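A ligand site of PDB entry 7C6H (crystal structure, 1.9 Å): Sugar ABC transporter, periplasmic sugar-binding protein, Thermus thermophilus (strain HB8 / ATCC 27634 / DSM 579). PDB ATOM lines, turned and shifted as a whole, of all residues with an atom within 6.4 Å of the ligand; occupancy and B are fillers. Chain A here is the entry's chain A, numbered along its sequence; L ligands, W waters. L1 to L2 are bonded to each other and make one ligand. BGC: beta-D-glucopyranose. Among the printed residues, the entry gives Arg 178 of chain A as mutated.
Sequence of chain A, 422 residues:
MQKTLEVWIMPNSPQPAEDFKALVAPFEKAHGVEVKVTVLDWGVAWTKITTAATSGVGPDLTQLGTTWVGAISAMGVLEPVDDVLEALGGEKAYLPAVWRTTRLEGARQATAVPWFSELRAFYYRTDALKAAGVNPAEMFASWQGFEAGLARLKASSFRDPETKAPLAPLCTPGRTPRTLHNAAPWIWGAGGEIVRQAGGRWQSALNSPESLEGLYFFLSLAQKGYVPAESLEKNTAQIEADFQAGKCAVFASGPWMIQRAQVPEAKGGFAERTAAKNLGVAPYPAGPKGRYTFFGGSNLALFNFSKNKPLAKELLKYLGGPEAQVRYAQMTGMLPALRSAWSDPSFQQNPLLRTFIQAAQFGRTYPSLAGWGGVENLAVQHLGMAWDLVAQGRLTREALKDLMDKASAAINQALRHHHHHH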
ATOM      1  N   PRO A  11       3.004 -24.955   8.834  1.00  0.00           N
ATOM      2  CA  PRO A  11       2.221 -23.714   8.909  1.00  0.00           C
ATOM      3  C   PRO A  11       3.109 -22.445   8.914  1.00  0.00           C
ATOM      4  O   PRO A  11       3.310 -21.862   9.922  1.00  0.00           O
ATOM      5  CB  PRO A  11       1.492 -23.851  10.249  1.00  0.00           C
ATOM      6  CG  PRO A  11       1.670 -25.302  10.690  1.00  0.00           C
ATOM      7  CD  PRO A  11       2.975 -25.704  10.104  1.00  0.00           C
ATOM      8  N   TRP A  42       4.279 -28.519  12.784  1.00  0.00           N
ATOM      9  CA  TRP A  42       5.724 -28.649  13.002  1.00  0.00           C
ATOM     10  C   TRP A  42       6.028 -29.837  13.901  1.00  0.00           C
ATOM     11  O   TRP A  42       7.009 -30.529  13.661  1.00  0.00           O
ATOM     12  CB  TRP A  42       6.263 -27.336  13.593  1.00  0.00           C
ATOM     13  CG  TRP A  42       6.661 -26.361  12.538  1.00  0.00           C
ATOM     14  CD1 TRP A  42       6.021 -25.217  12.148  1.00  0.00           C
ATOM     15  CD2 TRP A  42       7.835 -26.482  11.710  1.00  0.00           C
ATOM     16  NE1 TRP A  42       6.726 -24.629  11.123  1.00  0.00           N
ATOM     17  CE2 TRP A  42       7.841 -25.385  10.846  1.00  0.00           C
ATOM     18  CE3 TRP A  42       8.827 -27.456  11.589  1.00  0.00           C
ATOM     19  CZ2 TRP A  42       8.856 -25.210   9.903  1.00  0.00           C
ATOM     20  CZ3 TRP A  42       9.819 -27.301  10.646  1.00  0.00           C
ATOM     21  CH2 TRP A  42       9.830 -26.181   9.805  1.00  0.00           C
ATOM     22  N   LEU A  64      11.288 -29.243   4.438  1.00  0.00           N
ATOM     23  CA  LEU A  64      12.149 -29.700   5.542  1.00  0.00           C
ATOM     24  C   LEU A  64      12.701 -28.482   6.271  1.00  0.00           C
ATOM     25  O   LEU A  64      13.188 -27.577   5.580  1.00  0.00           O
ATOM     26  CB  LEU A  64      13.363 -30.459   4.975  1.00  0.00           C
ATOM     27  CG  LEU A  64      13.091 -31.761   4.195  1.00  0.00           C
ATOM     28  CD1 LEU A  64      14.432 -32.275   3.633  1.00  0.00           C
ATOM     29  CD2 LEU A  64      12.380 -32.727   5.107  1.00  0.00           C
ATOM     30  N   GLY A  65      12.675 -28.469   7.593  1.00  0.00           N
ATOM     31  CA  GLY A  65      13.534 -27.552   8.355  1.00  0.00           C
ATOM     32  C   GLY A  65      14.962 -27.682   7.850  1.00  0.00           C
ATOM     33  O   GLY A  65      15.422 -28.858   7.559  1.00  0.00           O
ATOM     34  N   THR A  66      15.738 -26.572   7.797  1.00  0.00           N
ATOM     35  CA  THR A  66      17.140 -26.739   7.414  1.00  0.00           C
ATOM     36  C   THR A  66      17.813 -27.814   8.278  1.00  0.00           C
ATOM     37  O   THR A  66      18.738 -28.486   7.751  1.00  0.00           O
ATOM     38  CB  THR A  66      17.860 -25.383   7.518  1.00  0.00           C
ATOM     39  OG1 THR A  66      17.630 -24.895   8.840  1.00  0.00           O
ATOM     40  CG2 THR A  66      17.429 -24.408   6.444  1.00  0.00           C
ATOM     41  N   THR A  67      17.520 -27.913   9.590  1.00  0.00           N
ATOM     42  CA  THR A  67      18.219 -28.836  10.525  1.00  0.00           C
ATOM     43  C   THR A  67      17.844 -30.298  10.253  1.00  0.00           C
ATOM     44  O   THR A  67      18.482 -31.154  10.884  1.00  0.00           O
ATOM     45  CB  THR A  67      18.009 -28.450  11.987  1.00  0.00           C
ATOM     46  OG1 THR A  67      16.628 -28.554  12.365  1.00  0.00           O
ATOM     47  CG2 THR A  67      18.535 -27.043  12.248  1.00  0.00           C
ATOM     48  N   TRP A  68      16.829 -30.574   9.415  1.00  0.00           N
ATOM     49  CA  TRP A  68      16.356 -31.948   9.083  1.00  0.00           C
ATOM     50  C   TRP A  68      17.020 -32.541   7.836  1.00  0.00           C
ATOM     51  O   TRP A  68      16.868 -33.787   7.545  1.00  0.00           O
ATOM     52  CB  TRP A  68      14.862 -31.841   8.837  1.00  0.00           C
ATOM     53  CG  TRP A  68      14.059 -31.498  10.040  1.00  0.00           C
ATOM     54  CD1 TRP A  68      14.440 -31.254  11.324  1.00  0.00           C
ATOM     55  CD2 TRP A  68      12.624 -31.409  10.027  1.00  0.00           C
ATOM     56  NE1 TRP A  68      13.331 -30.925  12.070  1.00  0.00           N
ATOM     57  CE2 TRP A  68      12.222 -31.075  11.318  1.00  0.00           C
ATOM     58  CE3 TRP A  68      11.681 -31.631   9.011  1.00  0.00           C
ATOM     59  CZ2 TRP A  68      10.876 -30.982  11.687  1.00  0.00           C
ATOM     60  CZ3 TRP A  68      10.356 -31.549   9.371  1.00  0.00           C
ATOM     61  CH2 TRP A  68       9.984 -31.197  10.674  1.00  0.00           C
ATOM     62  N   PHE A 116      13.116 -20.599   2.232  1.00  0.00           N
ATOM     63  CA  PHE A 116      13.053 -19.351   2.989  1.00  0.00           C
ATOM     64  C   PHE A 116      14.027 -19.443   4.141  1.00  0.00           C
ATOM     65  O   PHE A 116      14.275 -20.515   4.622  1.00  0.00           O
ATOM     66  CB  PHE A 116      11.619 -18.916   3.335  1.00  0.00           C
ATOM     67  CG  PHE A 116      10.904 -19.805   4.295  1.00  0.00           C
ATOM     68  CD1 PHE A 116      11.103 -19.700   5.652  1.00  0.00           C
ATOM     69  CD2 PHE A 116      10.001 -20.764   3.831  1.00  0.00           C
ATOM     70  CE1 PHE A 116      10.442 -20.553   6.550  1.00  0.00           C
ATOM     71  CE2 PHE A 116       9.321 -21.592   4.734  1.00  0.00           C
ATOM     72  CZ  PHE A 116       9.527 -21.481   6.087  1.00  0.00           C
ATOM     73  N   GLU A 118      15.124 -18.234   8.079  1.00  0.00           N
ATOM     74  CA  GLU A 118      14.904 -17.637   9.415  1.00  0.00           C
ATOM     75  C   GLU A 118      16.240 -17.041   9.864  1.00  0.00           C
ATOM     76  O   GLU A 118      17.305 -17.692   9.706  1.00  0.00           O
ATOM     77  CB  GLU A 118      14.299 -18.662  10.366  1.00  0.00           C
ATOM     78  CG  GLU A 118      14.059 -18.042  11.761  1.00  0.00           C
ATOM     79  CD  GLU A 118      13.501 -18.970  12.821  1.00  0.00           C
ATOM     80  OE1 GLU A 118      13.072 -20.197  12.463  1.00  0.00           O
ATOM     81  OE2 GLU A 118      13.570 -18.544  13.986  1.00  0.00           O
ATOM     82  N   ARG A 120      17.920 -14.069  13.023  1.00  0.00           N
ATOM     83  CA  ARG A 120      17.651 -13.344  14.267  1.00  0.00           C
ATOM     84  C   ARG A 120      18.521 -12.093  14.388  1.00  0.00           C
ATOM     85  O   ARG A 120      19.715 -12.104  14.085  1.00  0.00           O
ATOM     86  CB  ARG A 120      17.952 -14.234  15.457  1.00  0.00           C
ATOM     87  CG  ARG A 120      17.458 -15.667  15.254  1.00  0.00           C
ATOM     88  CD  ARG A 120      16.008 -15.632  15.487  1.00  0.00           C
ATOM     89  NE  ARG A 120      15.467 -17.010  15.538  1.00  0.00           N
ATOM     90  CZ  ARG A 120      15.449 -17.794  16.604  1.00  0.00           C
ATOM     91  NH1 ARG A 120      16.059 -17.428  17.730  1.00  0.00           N
ATOM     92  NH2 ARG A 120      14.857 -18.991  16.503  1.00  0.00           N
ATOM     93  N   ARG A 178      13.632 -24.570  21.445  1.00  0.00           N
ATOM     94  CA  ARG A 178      14.495 -23.888  20.430  1.00  0.00           C
ATOM     95  C   ARG A 178      15.499 -22.983  21.156  1.00  0.00           C
ATOM     96  O   ARG A 178      16.074 -22.075  20.549  1.00  0.00           O
ATOM     97  CB  ARG A 178      13.620 -23.128  19.437  1.00  0.00           C
ATOM     98  CG  ARG A 178      12.464 -23.926  18.886  1.00  0.00           C
ATOM     99  CD  ARG A 178      11.815 -23.229  17.724  1.00  0.00           C
ATOM    100  NE  ARG A 178      10.757 -22.316  18.153  1.00  0.00           N
ATOM    101  CZ  ARG A 178      10.547 -21.090  17.645  1.00  0.00           C
ATOM    102  NH1 ARG A 178      11.389 -20.566  16.753  1.00  0.00           N
ATOM    103  NH2 ARG A 178       9.481 -20.401  18.035  1.00  0.00           N
ATOM    104  N   HIS A 181      19.088 -22.181  19.570  1.00  0.00           N
ATOM    105  CA  HIS A 181      19.235 -21.133  18.522  1.00  0.00           C
ATOM    106  C   HIS A 181      19.549 -19.779  19.181  1.00  0.00           C
ATOM    107  O   HIS A 181      20.280 -18.974  18.515  1.00  0.00           O
ATOM    108  CB  HIS A 181      18.034 -20.989  17.616  1.00  0.00           C
ATOM    109  CG  HIS A 181      17.438 -22.263  17.126  1.00  0.00           C
ATOM    110  ND1 HIS A 181      18.219 -23.414  16.966  1.00  0.00           N
ATOM    111  CD2 HIS A 181      16.222 -22.528  16.610  1.00  0.00           C
ATOM    112  CE1 HIS A 181      17.434 -24.356  16.459  1.00  0.00           C
ATOM    113  NE2 HIS A 181      16.216 -23.843  16.206  1.00  0.00           N
ATOM    114  N   TRP A 256       9.632 -10.862  10.848  1.00  0.00           N
ATOM    115  CA  TRP A 256       8.144 -10.822  10.902  1.00  0.00           C
ATOM    116  C   TRP A 256       7.632  -9.724  11.855  1.00  0.00           C
ATOM    117  O   TRP A 256       6.491  -9.272  11.634  1.00  0.00           O
ATOM    118  CB  TRP A 256       7.583 -12.167  11.296  1.00  0.00           C
ATOM    119  CG  TRP A 256       8.188 -12.767  12.515  1.00  0.00           C
ATOM    120  CD1 TRP A 256       7.797 -12.560  13.808  1.00  0.00           C
ATOM    121  CD2 TRP A 256       9.258 -13.736  12.585  1.00  0.00           C
ATOM    122  NE1 TRP A 256       8.537 -13.313  14.656  1.00  0.00           N
ATOM    123  CE2 TRP A 256       9.453 -14.035  13.945  1.00  0.00           C
ATOM    124  CE3 TRP A 256      10.064 -14.366  11.631  1.00  0.00           C
ATOM    125  CZ2 TRP A 256      10.433 -14.918  14.391  1.00  0.00           C
ATOM    126  CZ3 TRP A 256      11.067 -15.205  12.059  1.00  0.00           C
ATOM    127  CH2 TRP A 256      11.226 -15.521  13.430  1.00  0.00           C
ATOM    128  N   PHE A 294      22.418 -16.126  13.715  1.00  0.00           N
ATOM    129  CA  PHE A 294      21.790 -17.446  13.576  1.00  0.00           C
ATOM    130  C   PHE A 294      20.904 -17.473  12.336  1.00  0.00           C
ATOM    131  O   PHE A 294      20.051 -16.555  12.127  1.00  0.00           O
ATOM    132  CB  PHE A 294      20.909 -17.799  14.777  1.00  0.00           C
ATOM    133  CG  PHE A 294      20.237 -19.124  14.560  1.00  0.00           C
ATOM    134  CD1 PHE A 294      20.928 -20.309  14.798  1.00  0.00           C
ATOM    135  CD2 PHE A 294      18.953 -19.186  14.057  1.00  0.00           C
ATOM    136  CE1 PHE A 294      20.318 -21.528  14.610  1.00  0.00           C
ATOM    137  CE2 PHE A 294      18.323 -20.406  13.883  1.00  0.00           C
ATOM    138  CZ  PHE A 294      19.013 -21.581  14.171  1.00  0.00           C
ATOM    139  N   PHE A 295      21.134 -18.487  11.497  1.00  0.00           N
ATOM    140  CA  PHE A 295      20.281 -18.847  10.358  1.00  0.00           C
ATOM    141  C   PHE A 295      19.627 -20.225  10.563  1.00  0.00           C
ATOM    142  O   PHE A 295      20.284 -21.243  10.950  1.00  0.00           O
ATOM    143  CB  PHE A 295      21.088 -18.859   9.071  1.00  0.00           C
ATOM    144  CG  PHE A 295      20.929 -17.599   8.267  1.00  0.00           C
ATOM    145  CD1 PHE A 295      21.425 -16.393   8.740  1.00  0.00           C
ATOM    146  CD2 PHE A 295      20.314 -17.633   7.036  1.00  0.00           C
ATOM    147  CE1 PHE A 295      21.264 -15.232   7.993  1.00  0.00           C
ATOM    148  CE2 PHE A 295      20.119 -16.473   6.304  1.00  0.00           C
ATOM    149  CZ  PHE A 295      20.615 -15.277   6.792  1.00  0.00           C
ATOM    150  N   GLY A 296      18.358 -20.261  10.177  1.00  0.00           N
ATOM    151  CA  GLY A 296      17.527 -21.488  10.000  1.00  0.00           C
ATOM    152  C   GLY A 296      16.658 -21.255   8.795  1.00  0.00           C
ATOM    153  O   GLY A 296      17.115 -20.549   7.837  1.00  0.00           O
ATOM    154  N   GLY A 297      15.455 -21.810   8.838  1.00  0.00           N
ATOM    155  CA  GLY A 297      14.448 -21.689   7.764  1.00  0.00           C
ATOM    156  C   GLY A 297      14.146 -23.071   7.241  1.00  0.00           C
ATOM    157  O   GLY A 297      14.292 -24.127   7.965  1.00  0.00           O
ATOM    158  N   SER A 298      13.623 -23.069   6.039  1.00  0.00           N
ATOM    159  CA  SER A 298      13.089 -24.299   5.429  1.00  0.00           C
ATOM    160  C   SER A 298      13.525 -24.376   3.979  1.00  0.00           C
ATOM    161  O   SER A 298      13.664 -23.329   3.264  1.00  0.00           O
ATOM    162  CB  SER A 298      11.600 -24.389   5.582  1.00  0.00           C
ATOM    163  OG  SER A 298      11.208 -24.674   6.908  1.00  0.00           O
ATOM    164  N   MET A 334       9.411 -14.032   6.573  1.00  0.00           N
ATOM    165  CA  MET A 334      10.814 -14.523   6.592  1.00  0.00           C
ATOM    166  C   MET A 334      11.657 -13.749   5.580  1.00  0.00           C
ATOM    167  O   MET A 334      11.117 -12.804   5.000  1.00  0.00           O
ATOM    168  CB  MET A 334      10.848 -16.025   6.301  1.00  0.00           C
ATOM    169  CG  MET A 334      10.117 -16.795   7.361  1.00  0.00           C
ATOM    170  SD  MET A 334      11.241 -17.243   8.714  1.00  0.00           S
ATOM    171  CE  MET A 334      10.064 -17.984   9.843  1.00  0.00           C
ATOM    172  N   GLU A 376      20.881 -31.808  19.081  1.00  0.00           N
ATOM    173  CA  GLU A 376      20.096 -30.647  19.547  1.00  0.00           C
ATOM    174  C   GLU A 376      19.217 -30.993  20.766  1.00  0.00           C
ATOM    175  O   GLU A 376      19.212 -30.244  21.711  1.00  0.00           O
ATOM    176  CB  GLU A 376      19.269 -30.106  18.367  1.00  0.00           C
ATOM    177  CG  GLU A 376      18.630 -28.742  18.700  1.00  0.00           C
ATOM    178  CD  GLU A 376      17.879 -28.083  17.544  1.00  0.00           C
ATOM    179  OE1 GLU A 376      18.263 -28.245  16.355  1.00  0.00           O
ATOM    180  OE2 GLU A 376      16.937 -27.351  17.861  1.00  0.00           O
HETATM  181  C2  BGC L   1       9.931 -21.486  13.242  1.00  0.00           C
HETATM  182  C3  BGC L   1      10.289 -22.947  13.087  1.00  0.00           C
HETATM  183  C4  BGC L   1       9.719 -23.713  14.241  1.00  0.00           C
HETATM  184  C5  BGC L   1       8.239 -23.446  14.343  1.00  0.00           C
HETATM  185  C6  BGC L   1       7.506 -24.065  15.531  1.00  0.00           C
HETATM  186  C1  BGC L   1       8.408 -21.316  13.341  1.00  0.00           C
HETATM  187  O1  BGC L   1       8.235 -19.934  13.617  1.00  0.00           O
HETATM  188  O2  BGC L   1      10.494 -20.749  12.174  1.00  0.00           O
HETATM  189  O3  BGC L   1      11.722 -23.053  13.095  1.00  0.00           O
HETATM  190  O4  BGC L   1      10.027 -25.103  14.110  1.00  0.00           O
HETATM  191  O5  BGC L   1       8.014 -22.026  14.505  1.00  0.00           O
HETATM  192  O6  BGC L   1       8.255 -23.841  16.742  1.00  0.00           O
HETATM  193  C2  BGC L   2      13.699 -23.511  11.884  1.00  0.00           C
HETATM  194  C3  BGC L   2      14.481 -24.580  11.109  1.00  0.00           C
HETATM  195  C4  BGC L   2      14.469 -25.931  11.850  1.00  0.00           C
HETATM  196  C5  BGC L   2      13.009 -26.290  12.221  1.00  0.00           C
HETATM  197  C6  BGC L   2      12.875 -27.634  12.944  1.00  0.00           C
HETATM  198  C1  BGC L   2      12.283 -24.024  12.250  1.00  0.00           C
HETATM  199  O2  BGC L   2      13.552 -22.425  10.990  1.00  0.00           O
HETATM  200  O3  BGC L   2      15.817 -24.070  10.872  1.00  0.00           O
HETATM  201  O4  BGC L   2      15.029 -26.965  11.038  1.00  0.00           O
HETATM  202  O5  BGC L   2      12.437 -25.228  13.025  1.00  0.00           O
HETATM  203  O6  BGC L   2      13.496 -27.573  14.207  1.00  0.00           O
HETATM  204  O   HOH W   1      14.842 -26.492  16.993  1.00  0.00           O
HETATM  205  O   HOH W   2      13.373 -21.420  15.231  1.00  0.00           O
HETATM  206  O   HOH W   3      16.369 -27.432  14.708  1.00  0.00           O
HETATM  207  O   HOH W   4      13.672 -24.733  15.689  1.00  0.00           O
HETATM  208  O   HOH W   5      11.588 -22.812   8.918  1.00  0.00           O
HETATM  209  O   HOH W   6       9.457 -27.134  15.909  1.00  0.00           O
HETATM  210  O   HOH W   7       9.256 -18.497  15.819  1.00  0.00           O
HETATM  211  O   HOH W   8       9.414 -21.476   9.677  1.00  0.00           O
HETATM  212  O   HOH W   9       8.777 -25.272  19.394  1.00  0.00           O
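N of Thr 67 is in hydrogen-bond range of O4 of BGC L2, 3.0 Å away.
OG1 of Thr 67 lies within hydrogen-bond range of O4 of BGC L2.
An oxygen (O2) of BGC L1 sits at hydrogen-bond distance from the side-chain carboxylate of Glu 118, at 2.7 Å.
An oxygen (O4) of BGC L2 sits at hydrogen-bond distance from the backbone NH of Thr 66 (3.3 Å).
An oxygen (O3) of BGC L2 is in hydrogen-bond range of the side-chain hydroxyl of Thr 66, 2.8 Å away.
The backbone NH (N) of Gly 297 lies within hydrogen-bond range of an oxygen (O2) of BGC L2 (2.9 Å).
O of Gly 297 sits close to O3 of BGC L2, at 3.3 Å.
NE of Arg 178 sits at hydrogen-bond distance from O6 of BGC L1, 3.3 Å away.
The backbone carbonyl oxygen of Glu 118 sits at hydrogen-bond distance from the backbone NH of Gly 296 (2.8 Å).
The guanidinium group (NH2) of Arg 120 lies within salt-bridge range of the side-chain carboxylate (OE2) of Glu 118.
N of Thr 66 is in hydrogen-bond range of O of Gly 297, 2.8 Å away.
Merely in contact with the ligand: Trp 42, Gly 65, Trp 68, Gly 296 and Met 334.
Hydrophobic or aromatic side chains that line the ligand: Trp 42, Trp 68 and Met 334.
Within 4 Å of the ligand: Trp 42, Gly 65, Thr 66, Thr 67, Trp 68, Glu 118, Arg 178, Gly 296, Gly 297 and Met 334.
Along chain A the residues within 4 Å of the ligand span positions 42 to 334.
Water W7 lies within hydrogen-bond range of an oxygen (O1) of BGC L1 (2.8 Å) and the guanidinium group (NH2) of Arg 178 (2.9 Å).
Water W5 lies within hydrogen-bond range of the side-chain hydroxyl (OG) of Ser 298 (2.8 Å), an oxygen (O2) of BGC L2 (2.9 Å) and the backbone carbonyl oxygen (O) of Gly 297 (3.2 Å).
Water W3 lies within hydrogen-bond range of OG1 of Thr 67 (2.6 Å), OE1 of Glu 376 (2.6 Å) and O6 of BGC L2 (2.9 Å).
Water W4 bridges a ring nitrogen (NE2) of His 181 (2.7 Å) and an oxygen (O5) of BGC L2 (3.0 Å).
Water W2 lies within hydrogen-bond range of the guanidinium group (NH1) of Arg 178, the side-chain carboxylate (OE1) of Glu 118, the guanidinium group (NH2) of Arg 120 and an oxygen (O3) of BGC L1.
Water W1 lies within hydrogen-bond range of OE2 of Glu 376 (2.4 Å), NE2 of His 181 (3.1 Å) and O6 of BGC L2 (3.3 Å).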
